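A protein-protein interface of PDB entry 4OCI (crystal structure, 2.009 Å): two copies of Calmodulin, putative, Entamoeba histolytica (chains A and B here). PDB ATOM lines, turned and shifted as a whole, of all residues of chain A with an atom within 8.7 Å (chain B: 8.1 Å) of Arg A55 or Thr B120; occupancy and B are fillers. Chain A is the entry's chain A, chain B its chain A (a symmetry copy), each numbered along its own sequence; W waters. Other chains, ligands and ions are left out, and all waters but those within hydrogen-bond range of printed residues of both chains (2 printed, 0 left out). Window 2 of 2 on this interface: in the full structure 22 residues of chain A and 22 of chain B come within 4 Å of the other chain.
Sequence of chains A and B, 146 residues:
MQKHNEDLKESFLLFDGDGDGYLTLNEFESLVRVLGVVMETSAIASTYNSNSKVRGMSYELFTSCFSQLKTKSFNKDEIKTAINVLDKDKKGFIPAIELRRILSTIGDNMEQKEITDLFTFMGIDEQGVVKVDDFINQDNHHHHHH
The backbone NH of Leu A25 is in hydrogen-bond range of the backbone carbonyl oxygen of His B145 (2.9 Å).
The side-chain amino group (NZ) of Lys A53 is in salt-bridge range of the side-chain carboxylate (OD2) of Asp B117, 3.98 Å away.
The side-chain hydroxyl (OH) of Tyr A48 sits at hydrogen-bond distance from the backbone carbonyl oxygen (O) of Leu A23, at 2.8 Å.
The side-chain carboxylate of Glu A27 is in hydrogen-bond range of the backbone NH of Thr A24, at 3.0 Å.
The side-chain hydroxyl (OG) of Ser A52 sits at hydrogen-bond distance from the backbone carbonyl oxygen (O) of Tyr A48 (2.8 Å).
O of Thr B116 lies within hydrogen-bond range of OG1 of Thr B120 (3.1 Å).
ND1 of His B146 sits at hydrogen-bond distance from O of His B142 (2.8 Å).
Among the printed residues, merely in contact across the chains: Thr A24 with His B145 (3.2 Å), Thr A24 with His B146 (3.95 Å), Tyr A48 with His B146 (3.1 Å), Val A54 with Glu B114 (3.8 Å), Val A54 with Leu B118 (3.9 Å), Val A54 with His B142 (2.9 Å), Arg A55 with Thr B120 (3.4 Å), Arg A55 with Phe B121 (3.9 Å), Arg A55 with His B146 (3.9 Å) and Gly A56 with His B146 (3.9 Å).
Of the printed residues of chain B, Tyr A48 touches His B146 (3.1 Å).
Of chain B, only Thr B120 (3.4 Å), Phe B121 (3.9 Å) and His B146 (3.9 Å) come within 4 Å of Arg A55.
Of chain B, only His B146 (3.9 Å) comes within 4 Å of Gly A56.
Printed residues of chain A within 4 Å of Leu B118: Val A54.
Of chain A, only Arg A55 (3.4 Å) comes within 4 Å of Thr B120.
Printed residues of chain A within 4 Å of His B142: Val A54.
The nearest residue of chain B that does not touch Arg A55 is His B142 (5.0 Å).
The nearest residue of chain A that does not touch Thr B120 is Val A54 (7.4 Å).
The nearest printed residue of chain B that does not touch Val A54 is Asp B117 (4.1 Å).
Hydrophobic or aromatic side chains of chain B that line the printed part of chain A: Leu B118, Phe B121, His B142 and His B146.
Along chain B the printed residues that touch a printed residue of chain A span positions 114 to 146.
Printed residues of chain A that touch a printed residue of chain B: Thr A24, Leu A25, Tyr A48, Lys A53, Val A54, Arg A55 and Gly A56.
Hydrophobic or aromatic side chains of chain A within 4 Å of the printed part of chain B: Leu A25, Tyr A48 and Val A54.
Among the printed residues, 12 pairs touch across the chains.
No position is printed for both chains.
Water W1 lies within hydrogen-bond range of O of Arg A55 and NE2 of His B146.
Water W2 bridges the side-chain hydroxyl of Ser A52 (2.8 Å) and the backbone carbonyl oxygen of His B146 (3.0 Å).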
ATOM      1  N   ASP A  16      34.717  20.241   6.268  1.00  0.00           N
ATOM      2  CA  ASP A  16      33.391  19.881   5.786  1.00  0.00           C
ATOM      3  C   ASP A  16      33.558  19.536   4.316  1.00  0.00           C
ATOM      4  O   ASP A  16      33.539  20.413   3.447  1.00  0.00           O
ATOM      5  CB  ASP A  16      32.420  21.055   5.986  1.00  0.00           C
ATOM      6  CG  ASP A  16      31.170  20.972   5.111  1.00  0.00           C
ATOM      7  OD1 ASP A  16      30.637  19.864   4.933  1.00  0.00           O
ATOM      8  OD2 ASP A  16      30.659  22.028   4.690  1.00  0.00           O
ATOM      9  N   ASP A  18      31.893  18.076   1.886  1.00  0.00           N
ATOM     10  CA  ASP A  18      30.933  18.203   0.843  1.00  0.00           C
ATOM     11  C   ASP A  18      30.305  19.624   0.721  1.00  0.00           C
ATOM     12  O   ASP A  18      29.321  19.796   0.023  1.00  0.00           O
ATOM     13  CB  ASP A  18      29.873  17.125   0.996  1.00  0.00           C
ATOM     14  CG  ASP A  18      29.021  17.329   2.261  1.00  0.00           C
ATOM     15  OD1 ASP A  18      29.338  18.190   3.095  1.00  0.00           O
ATOM     16  OD2 ASP A  18      28.013  16.635   2.426  1.00  0.00           O
ATOM     17  N   ASP A  20      28.369  21.532   2.624  1.00  0.00           N
ATOM     18  CA  ASP A  20      26.998  21.807   3.050  1.00  0.00           C
ATOM     19  C   ASP A  20      26.884  22.512   4.373  1.00  0.00           C
ATOM     20  O   ASP A  20      25.770  22.769   4.812  1.00  0.00           O
ATOM     21  CB  ASP A  20      26.117  20.550   3.024  1.00  0.00           C
ATOM     22  CG  ASP A  20      26.577  19.452   4.058  1.00  0.00           C
ATOM     23  OD1 ASP A  20      27.670  19.607   4.657  1.00  0.00           O
ATOM     24  OD2 ASP A  20      25.874  18.417   4.217  1.00  0.00           O
ATOM     25  N   GLY A  21      28.002  22.829   5.019  1.00  0.00           N
ATOM     26  CA  GLY A  21      28.005  23.446   6.386  1.00  0.00           C
ATOM     27  C   GLY A  21      27.821  22.480   7.584  1.00  0.00           C
ATOM     28  O   GLY A  21      27.472  22.929   8.705  1.00  0.00           O
ATOM     29  N   TYR A  22      28.025  21.181   7.381  1.00  0.00           N
ATOM     30  CA  TYR A  22      27.819  20.147   8.396  1.00  0.00           C
ATOM     31  C   TYR A  22      28.963  19.211   8.371  1.00  0.00           C
ATOM     32  O   TYR A  22      29.304  18.765   7.324  1.00  0.00           O
ATOM     33  CB  TYR A  22      26.534  19.304   8.145  1.00  0.00           C
ATOM     34  CG  TYR A  22      25.316  20.202   8.370  1.00  0.00           C
ATOM     35  CD1 TYR A  22      24.817  20.448   9.655  1.00  0.00           C
ATOM     36  CD2 TYR A  22      24.698  20.856   7.275  1.00  0.00           C
ATOM     37  CE1 TYR A  22      23.720  21.283   9.865  1.00  0.00           C
ATOM     38  CE2 TYR A  22      23.629  21.736   7.482  1.00  0.00           C
ATOM     39  CZ  TYR A  22      23.157  21.929   8.768  1.00  0.00           C
ATOM     40  OH  TYR A  22      22.105  22.763   8.960  1.00  0.00           O
ATOM     41  N   LEU A  23      29.472  18.796   9.536  1.00  0.00           N
ATOM     42  CA  LEU A  23      30.458  17.737   9.580  1.00  0.00           C
ATOM     43  C   LEU A  23      29.850  16.362   9.750  1.00  0.00           C
ATOM     44  O   LEU A  23      28.877  16.219  10.533  1.00  0.00           O
ATOM     45  CB  LEU A  23      31.429  18.002  10.761  1.00  0.00           C
ATOM     46  CG  LEU A  23      32.196  19.308  10.710  1.00  0.00           C
ATOM     47  CD1 LEU A  23      33.113  19.308  11.894  1.00  0.00           C
ATOM     48  CD2 LEU A  23      32.985  19.366   9.360  1.00  0.00           C
ATOM     49  N   THR A  24      30.389  15.374   9.020  1.00  0.00           N
ATOM     50  CA  THR A  24      30.122  13.948   9.329  1.00  0.00           C
ATOM     51  C   THR A  24      30.828  13.553  10.631  1.00  0.00           C
ATOM     52  O   THR A  24      31.605  14.319  11.158  1.00  0.00           O
ATOM     53  CB  THR A  24      30.593  13.017   8.264  1.00  0.00           C
ATOM     54  OG1 THR A  24      32.011  13.123   8.165  1.00  0.00           O
ATOM     55  CG2 THR A  24      29.939  13.334   6.900  1.00  0.00           C
ATOM     56  N   LEU A  25      30.574  12.337  11.145  1.00  0.00           N
ATOM     57  CA  LEU A  25      31.266  11.857  12.328  1.00  0.00           C
ATOM     58  C   LEU A  25      32.753  11.753  12.081  1.00  0.00           C
ATOM     59  O   LEU A  25      33.527  12.265  12.879  1.00  0.00           O
ATOM     60  CB  LEU A  25      30.722  10.443  12.655  1.00  0.00           C
ATOM     61  CG  LEU A  25      31.488   9.723  13.759  1.00  0.00           C
ATOM     62  CD1 LEU A  25      31.452  10.443  15.069  1.00  0.00           C
ATOM     63  CD2 LEU A  25      30.781   8.296  13.809  1.00  0.00           C
ATOM     64  N   GLU A  27      34.699  13.433   9.969  1.00  0.00           N
ATOM     65  CA  GLU A  27      35.240  14.792   9.872  1.00  0.00           C
ATOM     66  C   GLU A  27      35.325  15.477  11.218  1.00  0.00           C
ATOM     67  O   GLU A  27      36.308  16.177  11.478  1.00  0.00           O
ATOM     68  CB  GLU A  27      34.416  15.679   8.923  1.00  0.00           C
ATOM     69  CG  GLU A  27      34.549  15.183   7.440  1.00  0.00           C
ATOM     70  CD  GLU A  27      33.459  15.726   6.495  1.00  0.00           C
ATOM     71  OE1 GLU A  27      32.456  16.317   7.005  1.00  0.00           O
ATOM     72  OE2 GLU A  27      33.596  15.540   5.218  1.00  0.00           O
ATOM     73  N   TYR A  48      29.473  13.583  19.460  1.00  0.00           N
ATOM     74  CA  TYR A  48      28.843  13.811  18.135  1.00  0.00           C
ATOM     75  C   TYR A  48      27.368  13.323  18.142  1.00  0.00           C
ATOM     76  O   TYR A  48      26.464  14.022  17.657  1.00  0.00           O
ATOM     77  CB  TYR A  48      29.676  13.091  17.055  1.00  0.00           C
ATOM     78  CG  TYR A  48      29.152  13.364  15.668  1.00  0.00           C
ATOM     79  CD1 TYR A  48      29.622  14.429  14.931  1.00  0.00           C
ATOM     80  CD2 TYR A  48      28.092  12.567  15.098  1.00  0.00           C
ATOM     81  CE1 TYR A  48      29.105  14.703  13.603  1.00  0.00           C
ATOM     82  CE2 TYR A  48      27.565  12.830  13.807  1.00  0.00           C
ATOM     83  CZ  TYR A  48      28.101  13.885  13.059  1.00  0.00           C
ATOM     84  OH  TYR A  48      27.595  14.136  11.792  1.00  0.00           O
ATOM     85  N   ASN A  51      25.050  15.670  19.831  1.00  0.00           N
ATOM     86  CA  ASN A  51      25.035  17.081  19.399  1.00  0.00           C
ATOM     87  C   ASN A  51      25.104  17.163  17.879  1.00  0.00           C
ATOM     88  O   ASN A  51      25.984  17.820  17.291  1.00  0.00           O
ATOM     89  CB  ASN A  51      26.210  17.826  20.030  1.00  0.00           C
ATOM     90  CG  ASN A  51      26.115  17.854  21.549  1.00  0.00           C
ATOM     91  OD1 ASN A  51      25.376  18.647  22.130  1.00  0.00           O
ATOM     92  ND2 ASN A  51      26.827  16.956  22.194  1.00  0.00           N
ATOM     93  N   SER A  52      24.273  16.413  17.209  1.00  0.00           N
ATOM     94  CA  SER A  52      24.257  16.592  15.779  1.00  0.00           C
ATOM     95  C   SER A  52      22.798  16.496  15.396  1.00  0.00           C
ATOM     96  O   SER A  52      22.029  15.783  16.036  1.00  0.00           O
ATOM     97  CB  SER A  52      25.066  15.550  15.083  1.00  0.00           C
ATOM     98  OG  SER A  52      24.721  14.253  15.541  1.00  0.00           O
ATOM     99  N   LYS A  53      22.423  17.229  14.371  1.00  0.00           N
ATOM    100  CA  LYS A  53      21.103  17.054  13.745  1.00  0.00           C
ATOM    101  C   LYS A  53      21.217  15.911  12.783  1.00  0.00           C
ATOM    102  O   LYS A  53      22.335  15.374  12.502  1.00  0.00           O
ATOM    103  CB  LYS A  53      20.778  18.306  12.910  1.00  0.00           C
ATOM    104  CG  LYS A  53      21.077  19.736  13.562  1.00  0.00           C
ATOM    105  CD  LYS A  53      20.597  19.916  15.020  1.00  0.00           C
ATOM    106  CE  LYS A  53      19.092  20.293  15.140  1.00  0.00           C
ATOM    107  NZ  LYS A  53      18.214  19.158  14.584  1.00  0.00           N
ATOM    108  N   VAL A  54      20.096  15.603  12.155  1.00  0.00           N
ATOM    109  CA  VAL A  54      20.147  14.670  11.060  1.00  0.00           C
ATOM    110  C   VAL A  54      21.174  14.972   9.973  1.00  0.00           C
ATOM    111  O   VAL A  54      21.834  14.077   9.518  1.00  0.00           O
ATOM    112  CB  VAL A  54      18.708  14.402  10.432  1.00  0.00           C
ATOM    113  CG1 VAL A  54      18.860  13.661   9.158  1.00  0.00           C
ATOM    114  CG2 VAL A  54      17.874  13.578  11.448  1.00  0.00           C
ATOM    115  N   ARG A  55      21.295  16.229   9.537  1.00  0.00           N
ATOM    116  CA  ARG A  55      22.286  16.668   8.577  1.00  0.00           C
ATOM    117  C   ARG A  55      23.743  16.543   9.057  1.00  0.00           C
ATOM    118  O   ARG A  55      24.687  16.603   8.264  1.00  0.00           O
ATOM    119  CB  ARG A  55      21.987  18.156   8.208  1.00  0.00           C
ATOM    120  CG  ARG A  55      20.700  18.265   7.429  1.00  0.00           C
ATOM    121  CD  ARG A  55      20.589  19.632   6.813  1.00  0.00           C
ATOM    122  NE  ARG A  55      19.271  19.937   6.244  1.00  0.00           N
ATOM    123  CZ  ARG A  55      19.021  20.033   4.933  1.00  0.00           C
ATOM    124  NH1 ARG A  55      19.983  19.790   4.031  1.00  0.00           N
ATOM    125  NH2 ARG A  55      17.796  20.371   4.516  1.00  0.00           N
ATOM    126  N   GLY A  56      23.983  16.398  10.351  1.00  0.00           N
ATOM    127  CA  GLY A  56      25.377  16.373  10.765  1.00  0.00           C
ATOM    128  C   GLY A  56      25.573  17.447  11.829  1.00  0.00           C
ATOM    129  O   GLY A  56      24.626  17.865  12.480  1.00  0.00           O
ATOM    130  N   MET A  57      26.811  17.857  12.031  1.00  0.00           N
ATOM    131  CA  MET A  57      27.132  18.792  13.055  1.00  0.00           C
ATOM    132  C   MET A  57      27.382  20.191  12.458  1.00  0.00           C
ATOM    133  O   MET A  57      28.219  20.323  11.617  1.00  0.00           O
ATOM    134  CB  MET A  57      28.366  18.291  13.828  1.00  0.00           C
ATOM    135  CG  MET A  57      28.638  19.248  14.997  1.00  0.00           C
ATOM    136  SD  MET A  57      30.232  18.687  15.818  1.00  0.00           S
ATOM    137  CE  MET A  57      29.180  17.684  17.203  1.00  0.00           C
ATOM    138  N   SER A  58      26.639  21.201  12.881  1.00  0.00           N
ATOM    139  CA  SER A  58      26.748  22.568  12.335  1.00  0.00           C
ATOM    140  C   SER A  58      27.905  23.262  13.019  1.00  0.00           C
ATOM    141  O   SER A  58      28.502  22.714  13.958  1.00  0.00           O
ATOM    142  CB  SER A  58      25.438  23.330  12.639  1.00  0.00           C
ATOM    143  OG  SER A  58      25.427  23.578  14.038  1.00  0.00           O
ATOM    144  N   LEU A  61      27.088  24.059  16.896  1.00  0.00           N
ATOM    145  CA  LEU A  61      27.154  22.857  17.746  1.00  0.00           C
ATOM    146  C   LEU A  61      28.635  22.461  17.923  1.00  0.00           C
ATOM    147  O   LEU A  61      29.025  22.038  18.992  1.00  0.00           O
ATOM    148  CB  LEU A  61      26.416  21.688  17.071  1.00  0.00           C
ATOM    149  CG  LEU A  61      24.876  21.858  17.181  1.00  0.00           C
ATOM    150  CD1 LEU A  61      23.995  20.975  16.195  1.00  0.00           C
ATOM    151  CD2 LEU A  61      24.512  21.636  18.678  1.00  0.00           C
ATOM    152  N   ARG B 100       6.929   6.884   6.740  1.00  0.00           N
ATOM    153  CA  ARG B 100       6.833   7.502   8.080  1.00  0.00           C
ATOM    154  C   ARG B 100       6.193   6.574   9.057  1.00  0.00           C
ATOM    155  O   ARG B 100       6.722   6.399  10.156  1.00  0.00           O
ATOM    156  CB  ARG B 100       6.100   8.860   8.043  1.00  0.00           C
ATOM    157  CG  ARG B 100       5.944   9.592   9.394  1.00  0.00           C
ATOM    158  CD  ARG B 100       5.139  10.903   9.249  1.00  0.00           C
ATOM    159  NE  ARG B 100       5.918  11.997   8.610  1.00  0.00           N
ATOM    160  CZ  ARG B 100       6.811  12.759   9.236  1.00  0.00           C
ATOM    161  NH1 ARG B 100       7.141  12.552  10.531  1.00  0.00           N
ATOM    162  NH2 ARG B 100       7.433  13.720   8.561  1.00  0.00           N
ATOM    163  N   LYS B 113       9.845  14.453  14.536  1.00  0.00           N
ATOM    164  CA  LYS B 113      10.624  15.605  14.114  1.00  0.00           C
ATOM    165  C   LYS B 113      11.888  15.101  13.405  1.00  0.00           C
ATOM    166  O   LYS B 113      12.286  15.706  12.445  1.00  0.00           O
ATOM    167  CB  LYS B 113      10.964  16.543  15.311  1.00  0.00           C
ATOM    168  N   GLU B 114      12.497  14.009  13.853  1.00  0.00           N
ATOM    169  CA  GLU B 114      13.699  13.445  13.178  1.00  0.00           C
ATOM    170  C   GLU B 114      13.351  12.801  11.793  1.00  0.00           C
ATOM    171  O   GLU B 114      14.176  12.766  10.854  1.00  0.00           O
ATOM    172  CB  GLU B 114      14.535  12.467  14.084  1.00  0.00           C
ATOM    173  CG  GLU B 114      15.075  13.133  15.401  1.00  0.00           C
ATOM    174  CD  GLU B 114      15.570  12.163  16.503  1.00  0.00           C
ATOM    175  OE1 GLU B 114      15.188  10.963  16.541  1.00  0.00           O
ATOM    176  OE2 GLU B 114      16.348  12.641  17.368  1.00  0.00           O
ATOM    177  N   ILE B 115      12.128  12.280  11.689  1.00  0.00           N
ATOM    178  CA  ILE B 115      11.631  11.772  10.417  1.00  0.00           C
ATOM    179  C   ILE B 115      11.467  12.873   9.399  1.00  0.00           C
ATOM    180  O   ILE B 115      11.944  12.733   8.314  1.00  0.00           O
ATOM    181  CB  ILE B 115      10.394  10.914  10.588  1.00  0.00           C
ATOM    182  CG1 ILE B 115      10.848   9.694  11.396  1.00  0.00           C
ATOM    183  CG2 ILE B 115       9.865  10.471   9.209  1.00  0.00           C
ATOM    184  CD1 ILE B 115       9.776   8.698  11.850  1.00  0.00           C
ATOM    185  N   THR B 116      10.825  13.976   9.793  1.00  0.00           N
ATOM    186  CA  THR B 116      10.671  15.134   8.941  1.00  0.00           C
ATOM    187  C   THR B 116      12.061  15.646   8.487  1.00  0.00           C
ATOM    188  O   THR B 116      12.261  15.944   7.330  1.00  0.00           O
ATOM    189  CB  THR B 116       9.935  16.231   9.743  1.00  0.00           C
ATOM    190  OG1 THR B 116       8.699  15.697  10.227  1.00  0.00           O
ATOM    191  CG2 THR B 116       9.625  17.456   8.889  1.00  0.00           C
ATOM    192  N   ASP B 117      13.025  15.705   9.410  1.00  0.00           N
ATOM    193  CA  ASP B 117      14.346  16.244   9.094  1.00  0.00           C
ATOM    194  C   ASP B 117      15.076  15.319   8.152  1.00  0.00           C
ATOM    195  O   ASP B 117      15.731  15.766   7.252  1.00  0.00           O
ATOM    196  CB  ASP B 117      15.167  16.413  10.368  1.00  0.00           C
ATOM    197  CG  ASP B 117      14.666  17.614  11.275  1.00  0.00           C
ATOM    198  OD1 ASP B 117      13.754  18.406  10.841  1.00  0.00           O
ATOM    199  OD2 ASP B 117      15.184  17.729  12.438  1.00  0.00           O
ATOM    200  N   LEU B 118      14.935  14.021   8.355  1.00  0.00           N
ATOM    201  CA  LEU B 118      15.438  13.060   7.426  1.00  0.00           C
ATOM    202  C   LEU B 118      14.793  13.167   6.018  1.00  0.00           C
ATOM    203  O   LEU B 118      15.497  13.059   4.984  1.00  0.00           O
ATOM    204  CB  LEU B 118      15.174  11.686   8.010  1.00  0.00           C
ATOM    205  CG  LEU B 118      15.749  10.570   7.193  1.00  0.00           C
ATOM    206  CD1 LEU B 118      17.314  10.413   7.484  1.00  0.00           C
ATOM    207  CD2 LEU B 118      14.973   9.344   7.557  1.00  0.00           C
ATOM    208  N   PHE B 119      13.460  13.331   5.973  1.00  0.00           N
ATOM    209  CA  PHE B 119      12.766  13.438   4.675  1.00  0.00           C
ATOM    210  C   PHE B 119      13.187  14.714   3.967  1.00  0.00           C
ATOM    211  O   PHE B 119      13.414  14.682   2.791  1.00  0.00           O
ATOM    212  CB  PHE B 119      11.225  13.430   4.850  1.00  0.00           C
ATOM    213  CG  PHE B 119      10.622  12.033   5.078  1.00  0.00           C
ATOM    214  CD1 PHE B 119      11.395  10.928   5.207  1.00  0.00           C
ATOM    215  CD2 PHE B 119       9.230  11.876   5.135  1.00  0.00           C
ATOM    216  CE1 PHE B 119      10.806   9.614   5.411  1.00  0.00           C
ATOM    217  CE2 PHE B 119       8.636  10.609   5.337  1.00  0.00           C
ATOM    218  CZ  PHE B 119       9.443   9.471   5.471  1.00  0.00           C
ATOM    219  N   THR B 120      13.297  15.819   4.694  1.00  0.00           N
ATOM    220  CA  THR B 120      13.803  17.091   4.126  1.00  0.00           C
ATOM    221  C   THR B 120      15.217  16.972   3.585  1.00  0.00           C
ATOM    222  O   THR B 120      15.481  17.418   2.501  1.00  0.00           O
ATOM    223  CB  THR B 120      13.790  18.180   5.209  1.00  0.00           C
ATOM    224  OG1 THR B 120      12.410  18.486   5.500  1.00  0.00           O
ATOM    225  CG2 THR B 120      14.498  19.457   4.734  1.00  0.00           C
ATOM    226  N   PHE B 121      16.095  16.320   4.331  1.00  0.00           N
ATOM    227  CA  PHE B 121      17.453  16.054   3.926  1.00  0.00           C
ATOM    228  C   PHE B 121      17.515  15.259   2.574  1.00  0.00           C
ATOM    229  O   PHE B 121      18.306  15.587   1.641  1.00  0.00           O
ATOM    230  CB  PHE B 121      18.115  15.331   5.123  1.00  0.00           C
ATOM    231  CG  PHE B 121      19.461  14.787   4.862  1.00  0.00           C
ATOM    232  CD1 PHE B 121      20.521  15.627   4.590  1.00  0.00           C
ATOM    233  CD2 PHE B 121      19.691  13.424   4.927  1.00  0.00           C
ATOM    234  CE1 PHE B 121      21.810  15.107   4.384  1.00  0.00           C
ATOM    235  CE2 PHE B 121      20.953  12.894   4.677  1.00  0.00           C
ATOM    236  CZ  PHE B 121      22.027  13.756   4.432  1.00  0.00           C
ATOM    237  N   MET B 122      16.641  14.265   2.425  1.00  0.00           N
ATOM    238  CA  MET B 122      16.663  13.437   1.243  1.00  0.00           C
ATOM    239  C   MET B 122      15.806  13.954   0.121  1.00  0.00           C
ATOM    240  O   MET B 122      15.833  13.402  -0.968  1.00  0.00           O
ATOM    241  CB  MET B 122      16.239  12.016   1.594  1.00  0.00           C
ATOM    242  CG  MET B 122      17.365  11.292   2.289  1.00  0.00           C
ATOM    243  SD  MET B 122      16.730   9.519   2.752  1.00  0.00           S
ATOM    244  CE  MET B 122      18.256   8.921   3.876  1.00  0.00           C
ATOM    245  N   GLY B 123      15.021  14.972   0.380  1.00  0.00           N
ATOM    246  CA  GLY B 123      14.213  15.621  -0.671  1.00  0.00           C
ATOM    247  C   GLY B 123      12.880  14.894  -0.878  1.00  0.00           C
ATOM    248  O   GLY B 123      12.395  14.739  -1.996  1.00  0.00           O
ATOM    249  N   ILE B 124      12.327  14.378   0.211  1.00  0.00           N
ATOM    250  CA  ILE B 124      11.187  13.497   0.108  1.00  0.00           C
ATOM    251  C   ILE B 124      10.035  14.424   0.529  1.00  0.00           C
ATOM    252  O   ILE B 124      10.116  15.050   1.598  1.00  0.00           O
ATOM    253  CB  ILE B 124      11.349  12.299   1.078  1.00  0.00           C
ATOM    254  CG1 ILE B 124      12.367  11.273   0.543  1.00  0.00           C
ATOM    255  CG2 ILE B 124       9.948  11.664   1.387  1.00  0.00           C
ATOM    256  CD1 ILE B 124      12.606  10.137   1.505  1.00  0.00           C
ATOM    257  N   ASP B 125       8.976  14.532  -0.288  1.00  0.00           N
ATOM    258  CA  ASP B 125       7.803  15.297   0.214  1.00  0.00           C
ATOM    259  C   ASP B 125       6.841  14.429   0.921  1.00  0.00           C
ATOM    260  O   ASP B 125       6.551  13.330   0.474  1.00  0.00           O
ATOM    261  CB  ASP B 125       7.013  16.068  -0.844  1.00  0.00           C
ATOM    262  CG  ASP B 125       5.898  16.999  -0.185  1.00  0.00           C
ATOM    263  OD1 ASP B 125       6.267  18.054   0.476  1.00  0.00           O
ATOM    264  OD2 ASP B 125       4.653  16.682  -0.301  1.00  0.00           O
ATOM    265  N   GLU B 126       6.262  14.984   1.969  1.00  0.00           N
ATOM    266  CA  GLU B 126       5.284  14.313   2.835  1.00  0.00           C
ATOM    267  C   GLU B 126       4.033  13.770   2.134  1.00  0.00           C
ATOM    268  O   GLU B 126       3.492  12.757   2.536  1.00  0.00           O
ATOM    269  CB  GLU B 126       4.831  15.305   3.934  1.00  0.00           C
ATOM    270  CG  GLU B 126       4.465  14.615   5.254  1.00  0.00           C
ATOM    271  CD  GLU B 126       5.485  13.531   5.722  1.00  0.00           C
ATOM    272  OE1 GLU B 126       6.685  13.880   5.915  1.00  0.00           O
ATOM    273  OE2 GLU B 126       5.046  12.354   5.915  1.00  0.00           O
ATOM    274  N   HIS B 142      24.010   7.150   5.062  1.00  0.00           N
ATOM    275  CA  HIS B 142      23.931   8.120   6.095  1.00  0.00           C
ATOM    276  C   HIS B 142      24.393   7.527   7.460  1.00  0.00           C
ATOM    277  O   HIS B 142      25.226   8.118   8.167  1.00  0.00           O
ATOM    278  CB  HIS B 142      22.491   8.569   6.277  1.00  0.00           C
ATOM    279  CG  HIS B 142      22.340   9.530   7.395  1.00  0.00           C
ATOM    280  ND1 HIS B 142      22.717  10.855   7.273  1.00  0.00           N
ATOM    281  CD2 HIS B 142      21.870   9.364   8.656  1.00  0.00           C
ATOM    282  CE1 HIS B 142      22.515  11.455   8.435  1.00  0.00           C
ATOM    283  NE2 HIS B 142      22.002  10.576   9.285  1.00  0.00           N
ATOM    284  N   HIS B 145      28.123   7.143   8.221  1.00  0.00           N
ATOM    285  CA  HIS B 145      28.904   8.404   8.361  1.00  0.00           C
ATOM    286  C   HIS B 145      28.500   9.391   9.442  1.00  0.00           C
ATOM    287  O   HIS B 145      29.130  10.466   9.546  1.00  0.00           O
ATOM    288  CB  HIS B 145      28.966   9.093   7.020  1.00  0.00           C
ATOM    289  CG  HIS B 145      29.712   8.283   6.012  1.00  0.00           C
ATOM    290  ND1 HIS B 145      29.106   7.293   5.259  1.00  0.00           N
ATOM    291  CD2 HIS B 145      31.015   8.262   5.671  1.00  0.00           C
ATOM    292  CE1 HIS B 145      30.005   6.706   4.485  1.00  0.00           C
ATOM    293  NE2 HIS B 145      31.166   7.300   4.689  1.00  0.00           N
ATOM    294  N   HIS B 146      27.515   9.002  10.252  1.00  0.00           N
ATOM    295  CA  HIS B 146      26.930   9.805  11.325  1.00  0.00           C
ATOM    296  C   HIS B 146      26.716   9.018  12.652  1.00  0.00           C
ATOM    297  O   HIS B 146      26.083   9.720  13.547  1.00  0.00           O
ATOM    298  CB  HIS B 146      25.567  10.483  10.831  1.00  0.00           C
ATOM    299  CG  HIS B 146      25.767  11.364   9.625  1.00  0.00           C
ATOM    300  ND1 HIS B 146      25.864  10.852   8.343  1.00  0.00           N
ATOM    301  CD2 HIS B 146      26.005  12.693   9.514  1.00  0.00           C
ATOM    302  CE1 HIS B 146      26.135  11.843   7.498  1.00  0.00           C
ATOM    303  NE2 HIS B 146      26.216  12.969   8.179  1.00  0.00           N
HETATM  304  O   HOH W   1      26.908  15.594   7.594  1.00  0.00           O
HETATM  305  O   HOH W   2      24.104  11.768  14.431  1.00  0.00           O
